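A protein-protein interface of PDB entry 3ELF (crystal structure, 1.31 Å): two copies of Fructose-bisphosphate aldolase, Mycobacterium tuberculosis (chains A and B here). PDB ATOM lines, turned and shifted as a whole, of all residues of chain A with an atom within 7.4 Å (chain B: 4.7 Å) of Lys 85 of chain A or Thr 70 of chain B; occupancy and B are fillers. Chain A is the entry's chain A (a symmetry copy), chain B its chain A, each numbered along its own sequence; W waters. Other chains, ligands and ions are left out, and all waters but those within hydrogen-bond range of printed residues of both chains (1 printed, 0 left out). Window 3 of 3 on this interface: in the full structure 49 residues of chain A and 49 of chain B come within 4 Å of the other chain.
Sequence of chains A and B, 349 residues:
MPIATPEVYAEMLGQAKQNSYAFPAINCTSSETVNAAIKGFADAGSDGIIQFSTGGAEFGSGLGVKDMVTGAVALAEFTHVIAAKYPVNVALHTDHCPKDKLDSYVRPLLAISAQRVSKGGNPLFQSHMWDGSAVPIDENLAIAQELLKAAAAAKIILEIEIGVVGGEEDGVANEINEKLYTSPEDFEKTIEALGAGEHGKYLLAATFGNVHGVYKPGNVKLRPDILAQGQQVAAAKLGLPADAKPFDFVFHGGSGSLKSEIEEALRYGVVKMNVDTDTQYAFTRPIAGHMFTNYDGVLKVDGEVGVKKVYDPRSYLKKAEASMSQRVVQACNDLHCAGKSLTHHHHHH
The backbone NH of Asp 67 of chain B sits at hydrogen-bond distance from the side-chain hydroxyl of Ser 61 of chain B (2.9 Å).
OD2 of Asp 67 of chain B is in hydrogen-bond range of OG1 of Thr 70 of chain B (2.8 Å).
Among the printed residues, pairs that only touch across the chains: Tyr 86 of chain A with Val 65 of chain B (3.4 Å), Phe 78 of chain A with Ala 74 of chain B (3.5 Å), Lys 85 of chain A with Thr 70 of chain B (3.6 Å), Val 81 of chain A with Thr 70 of chain B (3.7 Å), Val 81 of chain A with Ala 74 of chain B (3.7 Å), Asn 35 of chain A with Ser 61 of chain B (3.7 Å), Ile 82 of chain A with Ala 74 of chain B (3.8 Å), Ile 82 of chain A with Ser 61 of chain B (3.8 Å), Lys 85 of chain A with Val 65 of chain B (3.98 Å) and Ile 82 of chain A with Thr 70 of chain B (3.98 Å).
Printed residues of chain B within 4 Å of Val 81 of chain A: Thr 70 and Ala 74.
Ala 84 of chain A touches none of the printed residues of chain B.
Lys 85 of chain A touches just these residues of chain B: Val 65 and Thr 70.
Pro 87 of chain A touches none of the printed residues of chain B.
Of the printed residues of chain A, Val 65 of chain B touches Lys 85 and Tyr 86.
Of the printed residues of chain A, Thr 70 of chain B touches Val 81, Ile 82 and Lys 85.
Of the printed residues of chain A, Ala 74 of chain B touches Phe 78 (3.5 Å), Val 81 (3.7 Å) and Ile 82 (3.8 Å).
The nearest printed residue of chain B that does not touch Ile 82 of chain A is Val 65 of chain B (4.7 Å).
Printed residues of chain A that touch a printed residue of chain B: Asn 35, Phe 78, Val 81, Ile 82, Lys 85 and Tyr 86.
Hydrophobic or aromatic side chains of chain A that line the printed part of chain B: Phe 78, Val 81, Ile 82 and Tyr 86.
No position is printed for both chains.
Of the 10 pairs that touch across the chains among the printed residues, none has its exchanged pair printed and touching as well.
Water W1 lies within hydrogen-bond range of the backbone carbonyl oxygen (O) of Ser 61 of chain B (2.7 Å), the side-chain hydroxyl (OH) of Tyr 86 of chain A (2.7 Å) and the side-chain amide oxygen (OD1) of Asn 35 of chain A (2.8 Å).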
ATOM      1  N   PRO A   2      35.538  16.277  -7.641  1.00  0.00           N
ATOM      2  CA  PRO A   2      34.984  17.626  -7.762  1.00  0.00           C
ATOM      3  C   PRO A   2      34.254  17.798  -9.082  1.00  0.00           C
ATOM      4  O   PRO A   2      34.432  16.986  -9.997  1.00  0.00           O
ATOM      5  CB  PRO A   2      36.234  18.523  -7.738  1.00  0.00           C
ATOM      6  CG  PRO A   2      37.375  17.619  -8.085  1.00  0.00           C
ATOM      7  CD  PRO A   2      37.002  16.306  -7.480  1.00  0.00           C
ATOM      8  N   ILE A   3      33.431  18.836  -9.189  1.00  0.00           N
ATOM      9  CA  ILE A   3      32.955  19.279 -10.496  1.00  0.00           C
ATOM     10  C   ILE A   3      34.184  19.698 -11.309  1.00  0.00           C
ATOM     11  O   ILE A   3      35.102  20.328 -10.783  1.00  0.00           O
ATOM     12  CB  ILE A   3      31.963  20.467 -10.377  1.00  0.00           C
ATOM     13  CG1 ILE A   3      30.671  20.033  -9.674  1.00  0.00           C
ATOM     14  CG2 ILE A   3      31.657  21.091 -11.760  1.00  0.00           C
ATOM     15  CD1 ILE A   3      29.803  19.060 -10.476  1.00  0.00           C
ATOM     16  N   ASN A  35      23.772  10.165  -8.577  1.00  0.00           N
ATOM     17  CA  ASN A  35      24.603   9.460  -7.612  1.00  0.00           C
ATOM     18  C   ASN A  35      25.178   8.174  -8.207  1.00  0.00           C
ATOM     19  O   ASN A  35      26.354   7.858  -7.990  1.00  0.00           O
ATOM     20  CB  ASN A  35      23.810   9.158  -6.337  1.00  0.00           C
ATOM     21  CG  ASN A  35      23.711  10.357  -5.416  1.00  0.00           C
ATOM     22  OD1 ASN A  35      24.559  11.250  -5.450  1.00  0.00           O
ATOM     23  ND2 ASN A  35      22.682  10.376  -4.583  1.00  0.00           N
ATOM     24  N   ILE A  38      28.036   9.085 -10.838  1.00  0.00           N
ATOM     25  CA  ILE A  38      29.284   9.542 -10.237  1.00  0.00           C
ATOM     26  C   ILE A  38      29.993   8.405  -9.507  1.00  0.00           C
ATOM     27  O   ILE A  38      31.211   8.251  -9.617  1.00  0.00           O
ATOM     28  CB  ILE A  38      29.087  10.746  -9.301  1.00  0.00           C
ATOM     29  CG1 ILE A  38      28.485  11.917 -10.067  1.00  0.00           C
ATOM     30  CG2 ILE A  38      30.422  11.177  -8.719  1.00  0.00           C
ATOM     31  CD1 ILE A  38      28.132  13.106  -9.178  1.00  0.00           C
ATOM     32  N   PHE A  78      22.348  20.142  -7.027  1.00  0.00           N
ATOM     33  CA  PHE A  78      22.505  18.884  -6.323  1.00  0.00           C
ATOM     34  C   PHE A  78      23.864  18.259  -6.660  1.00  0.00           C
ATOM     35  O   PHE A  78      24.619  17.869  -5.768  1.00  0.00           O
ATOM     36  CB  PHE A  78      21.358  17.931  -6.697  1.00  0.00           C
ATOM     37  CG  PHE A  78      21.522  16.543  -6.149  1.00  0.00           C
ATOM     38  CD1 PHE A  78      21.049  16.225  -4.882  1.00  0.00           C
ATOM     39  CD2 PHE A  78      22.144  15.554  -6.907  1.00  0.00           C
ATOM     40  CE1 PHE A  78      21.227  14.940  -4.361  1.00  0.00           C
ATOM     41  CE2 PHE A  78      22.313  14.280  -6.394  1.00  0.00           C
ATOM     42  CZ  PHE A  78      21.853  13.974  -5.122  1.00  0.00           C
ATOM     43  N   THR A  79      24.166  18.174  -7.954  1.00  0.00           N
ATOM     44  CA  THR A  79      25.386  17.518  -8.430  1.00  0.00           C
ATOM     45  C   THR A  79      26.651  18.226  -7.943  1.00  0.00           C
ATOM     46  O   THR A  79      27.643  17.568  -7.622  1.00  0.00           O
ATOM     47  CB  THR A  79      25.385  17.416  -9.965  1.00  0.00           C
ATOM     48  OG1 THR A  79      24.190  16.752 -10.387  1.00  0.00           O
ATOM     49  CG2 THR A  79      26.585  16.621 -10.465  1.00  0.00           C
ATOM     50  N   HIS A  80      26.607  19.555  -7.872  1.00  0.00           N
ATOM     51  CA  HIS A  80      27.755  20.314  -7.369  1.00  0.00           C
ATOM     52  C   HIS A  80      28.105  19.908  -5.942  1.00  0.00           C
ATOM     53  O   HIS A  80      29.277  19.767  -5.610  1.00  0.00           O
ATOM     54  CB  HIS A  80      27.521  21.830  -7.467  1.00  0.00           C
ATOM     55  CG  HIS A  80      27.823  22.398  -8.823  1.00  0.00           C
ATOM     56  ND1 HIS A  80      28.902  23.222  -9.070  1.00  0.00           N
ATOM     57  CD2 HIS A  80      27.197  22.239 -10.011  1.00  0.00           C
ATOM     58  CE1 HIS A  80      28.917  23.553 -10.350  1.00  0.00           C
ATOM     59  NE2 HIS A  80      27.893  22.968 -10.944  1.00  0.00           N
ATOM     60  N   VAL A  81      27.092  19.685  -5.108  1.00  0.00           N
ATOM     61  CA  VAL A  81      27.330  19.305  -3.718  1.00  0.00           C
ATOM     62  C   VAL A  81      27.906  17.889  -3.662  1.00  0.00           C
ATOM     63  O   VAL A  81      28.889  17.640  -2.966  1.00  0.00           O
ATOM     64  CB  VAL A  81      26.039  19.417  -2.872  1.00  0.00           C
ATOM     65  CG1 VAL A  81      26.261  18.918  -1.455  1.00  0.00           C
ATOM     66  CG2 VAL A  81      25.545  20.857  -2.841  1.00  0.00           C
ATOM     67  N   ILE A  82      27.301  16.965  -4.404  1.00  0.00           N
ATOM     68  CA  ILE A  82      27.741  15.569  -4.399  1.00  0.00           C
ATOM     69  C   ILE A  82      29.164  15.400  -4.954  1.00  0.00           C
ATOM     70  O   ILE A  82      30.005  14.728  -4.346  1.00  0.00           O
ATOM     71  CB  ILE A  82      26.756  14.681  -5.208  1.00  0.00           C
ATOM     72  CG1 ILE A  82      25.344  14.698  -4.589  1.00  0.00           C
ATOM     73  CG2 ILE A  82      27.291  13.254  -5.349  1.00  0.00           C
ATOM     74  CD1 ILE A  82      25.261  14.237  -3.146  1.00  0.00           C
ATOM     75  N   ALA A  83      29.432  16.016  -6.104  1.00  0.00           N
ATOM     76  CA  ALA A  83      30.693  15.778  -6.811  1.00  0.00           C
ATOM     77  C   ALA A  83      31.907  16.243  -6.013  1.00  0.00           C
ATOM     78  O   ALA A  83      33.003  15.705  -6.172  1.00  0.00           O
ATOM     79  CB  ALA A  83      30.669  16.416  -8.184  1.00  0.00           C
ATOM     80  N   ALA A  84      31.695  17.216  -5.129  1.00  0.00           N
ATOM     81  CA  ALA A  84      32.767  17.714  -4.265  1.00  0.00           C
ATOM     82  C   ALA A  84      33.310  16.625  -3.338  1.00  0.00           C
ATOM     83  O   ALA A  84      34.428  16.740  -2.828  1.00  0.00           O
ATOM     84  CB  ALA A  84      32.287  18.915  -3.457  1.00  0.00           C
ATOM     85  N   LYS A  85      32.524  15.565  -3.132  1.00  0.00           N
ATOM     86  CA  LYS A  85      32.896  14.490  -2.208  1.00  0.00           C
ATOM     87  C   LYS A  85      33.572  13.297  -2.889  1.00  0.00           C
ATOM     88  O   LYS A  85      33.880  12.296  -2.233  1.00  0.00           O
ATOM     89  CB  LYS A  85      31.671  14.025  -1.401  1.00  0.00           C
ATOM     90  CG  LYS A  85      31.038  15.116  -0.530  1.00  0.00           C
ATOM     91  CD  LYS A  85      31.998  15.694   0.500  1.00  0.00           C
ATOM     92  CE  LYS A  85      32.187  14.761   1.681  1.00  0.00           C
ATOM     93  NZ  LYS A  85      33.059  15.376   2.724  1.00  0.00           N
ATOM     94  N   TYR A  86      33.811  13.411  -4.191  1.00  0.00           N
ATOM     95  CA  TYR A  86      34.471  12.347  -4.946  1.00  0.00           C
ATOM     96  C   TYR A  86      35.802  12.809  -5.533  1.00  0.00           C
ATOM     97  O   TYR A  86      35.909  13.960  -5.968  1.00  0.00           O
ATOM     98  CB  TYR A  86      33.586  11.910  -6.099  1.00  0.00           C
ATOM     99  CG  TYR A  86      32.413  11.051  -5.726  1.00  0.00           C
ATOM    100  CD1 TYR A  86      32.536   9.665  -5.655  1.00  0.00           C
ATOM    101  CD2 TYR A  86      31.161  11.618  -5.498  1.00  0.00           C
ATOM    102  CE1 TYR A  86      31.445   8.862  -5.364  1.00  0.00           C
ATOM    103  CE2 TYR A  86      30.067  10.827  -5.197  1.00  0.00           C
ATOM    104  CZ  TYR A  86      30.215   9.450  -5.131  1.00  0.00           C
ATOM    105  OH  TYR A  86      29.138   8.643  -4.843  1.00  0.00           O
ATOM    106  N   PRO A  87      36.816  11.930  -5.560  1.00  0.00           N
ATOM    107  CA  PRO A  87      38.110  12.415  -6.044  1.00  0.00           C
ATOM    108  C   PRO A  87      38.185  12.714  -7.548  1.00  0.00           C
ATOM    109  O   PRO A  87      39.085  13.436  -7.960  1.00  0.00           O
ATOM    110  CB  PRO A  87      39.076  11.291  -5.651  1.00  0.00           C
ATOM    111  CG  PRO A  87      38.232  10.074  -5.575  1.00  0.00           C
ATOM    112  CD  PRO A  87      36.872  10.519  -5.128  1.00  0.00           C
ATOM    113  N   VAL A  88      37.233  12.212  -8.334  1.00  0.00           N
ATOM    114  CA  VAL A  88      37.273  12.274  -9.803  1.00  0.00           C
ATOM    115  C   VAL A  88      36.600  13.551 -10.277  1.00  0.00           C
ATOM    116  O   VAL A  88      35.885  14.194  -9.505  1.00  0.00           O
ATOM    117  CB  VAL A  88      36.589  11.046 -10.461  1.00  0.00           C
ATOM    118  CG1 VAL A  88      37.331   9.755 -10.122  1.00  0.00           C
ATOM    119  CG2 VAL A  88      35.103  10.945 -10.068  1.00  0.00           C
ATOM    120  N   SER B  61      22.933  11.198  -0.268  1.00  0.00           N
ATOM    121  CA  SER B  61      24.338  11.449  -0.596  1.00  0.00           C
ATOM    122  C   SER B  61      24.934  10.405  -1.536  1.00  0.00           C
ATOM    123  O   SER B  61      26.021  10.623  -2.065  1.00  0.00           O
ATOM    124  CB  SER B  61      25.194  11.557   0.671  1.00  0.00           C
ATOM    125  OG  SER B  61      25.451  10.292   1.250  1.00  0.00           O
ATOM    126  N   VAL B  65      29.201   7.942  -1.030  1.00  0.00           N
ATOM    127  CA  VAL B  65      29.512   9.000  -0.058  1.00  0.00           C
ATOM    128  C   VAL B  65      29.039   8.617   1.351  1.00  0.00           C
ATOM    129  O   VAL B  65      29.826   8.629   2.305  1.00  0.00           O
ATOM    130  CB  VAL B  65      28.921  10.369  -0.491  1.00  0.00           C
ATOM    131  CG1 VAL B  65      29.245  11.457   0.525  1.00  0.00           C
ATOM    132  CG2 VAL B  65      29.430  10.771  -1.871  1.00  0.00           C
ATOM    133  N   ASP B  67      27.210  10.195   3.566  1.00  0.00           N
ATOM    134  CA  ASP B  67      27.460  11.289   4.500  1.00  0.00           C
ATOM    135  C   ASP B  67      26.179  12.089   4.679  1.00  0.00           C
ATOM    136  O   ASP B  67      25.639  12.645   3.723  1.00  0.00           O
ATOM    137  CB  ASP B  67      28.570  12.207   3.997  1.00  0.00           C
ATOM    138  CG  ASP B  67      28.927  13.277   5.004  1.00  0.00           C
ATOM    139  OD1 ASP B  67      29.507  12.933   6.053  1.00  0.00           O
ATOM    140  OD2 ASP B  67      28.610  14.455   4.759  1.00  0.00           O
ATOM    141  N   MET B  68      25.708  12.153   5.918  1.00  0.00           N
ATOM    142  CA  MET B  68      24.451  12.817   6.241  1.00  0.00           C
ATOM    143  C   MET B  68      24.440  14.294   5.872  1.00  0.00           C
ATOM    144  O   MET B  68      23.477  14.775   5.281  1.00  0.00           O
ATOM    145  CB  MET B  68      24.141  12.677   7.728  1.00  0.00           C
ATOM    146  CG  MET B  68      23.854  11.273   8.185  1.00  0.00           C
ATOM    147  SD  MET B  68      23.684  11.211   9.977  1.00  0.00           S
ATOM    148  CE  MET B  68      25.381  11.381  10.518  1.00  0.00           C
ATOM    149  N   VAL B  69      25.497  15.021   6.230  1.00  0.00           N
ATOM    150  CA  VAL B  69      25.544  16.445   5.908  1.00  0.00           C
ATOM    151  C   VAL B  69      25.499  16.672   4.401  1.00  0.00           C
ATOM    152  O   VAL B  69      24.713  17.482   3.926  1.00  0.00           O
ATOM    153  CB  VAL B  69      26.759  17.145   6.552  1.00  0.00           C
ATOM    154  CG1 VAL B  69      26.899  18.575   6.042  1.00  0.00           C
ATOM    155  CG2 VAL B  69      26.602  17.162   8.072  1.00  0.00           C
ATOM    156  N   THR B  70      26.306  15.923   3.649  1.00  0.00           N
ATOM    157  CA  THR B  70      26.330  16.055   2.194  1.00  0.00           C
ATOM    158  C   THR B  70      24.946  15.822   1.590  1.00  0.00           C
ATOM    159  O   THR B  70      24.492  16.598   0.747  1.00  0.00           O
ATOM    160  CB  THR B  70      27.343  15.076   1.573  1.00  0.00           C
ATOM    161  OG1 THR B  70      28.643  15.341   2.106  1.00  0.00           O
ATOM    162  CG2 THR B  70      27.399  15.228   0.062  1.00  0.00           C
ATOM    163  N   GLY B  71      24.272  14.754   2.018  1.00  0.00           N
ATOM    164  CA  GLY B  71      22.963  14.413   1.462  1.00  0.00           C
ATOM    165  C   GLY B  71      21.919  15.454   1.801  1.00  0.00           C
ATOM    166  O   GLY B  71      21.121  15.849   0.949  1.00  0.00           O
ATOM    167  N   ALA B  72      21.926  15.925   3.047  1.00  0.00           N
ATOM    168  CA  ALA B  72      20.969  16.943   3.460  1.00  0.00           C
ATOM    169  C   ALA B  72      21.198  18.257   2.712  1.00  0.00           C
ATOM    170  O   ALA B  72      20.246  18.889   2.262  1.00  0.00           O
ATOM    171  CB  ALA B  72      21.031  17.157   4.961  1.00  0.00           C
ATOM    172  N   VAL B  73      22.458  18.663   2.566  1.00  0.00           N
ATOM    173  CA  VAL B  73      22.765  19.893   1.837  1.00  0.00           C
ATOM    174  C   VAL B  73      22.391  19.767   0.363  1.00  0.00           C
ATOM    175  O   VAL B  73      21.774  20.667  -0.198  1.00  0.00           O
ATOM    176  CB  VAL B  73      24.245  20.318   2.015  1.00  0.00           C
ATOM    177  CG1 VAL B  73      24.599  21.508   1.119  1.00  0.00           C
ATOM    178  CG2 VAL B  73      24.512  20.664   3.476  1.00  0.00           C
ATOM    179  N   ALA B  74      22.741  18.643  -0.258  1.00  0.00           N
ATOM    180  CA  ALA B  74      22.467  18.450  -1.680  1.00  0.00           C
ATOM    181  C   ALA B  74      20.967  18.479  -1.949  1.00  0.00           C
ATOM    182  O   ALA B  74      20.495  19.144  -2.881  1.00  0.00           O
ATOM    183  CB  ALA B  74      23.069  17.146  -2.155  1.00  0.00           C
HETATM  184  O   HOH W   1      26.888  10.084  -4.547  1.00  0.00           O
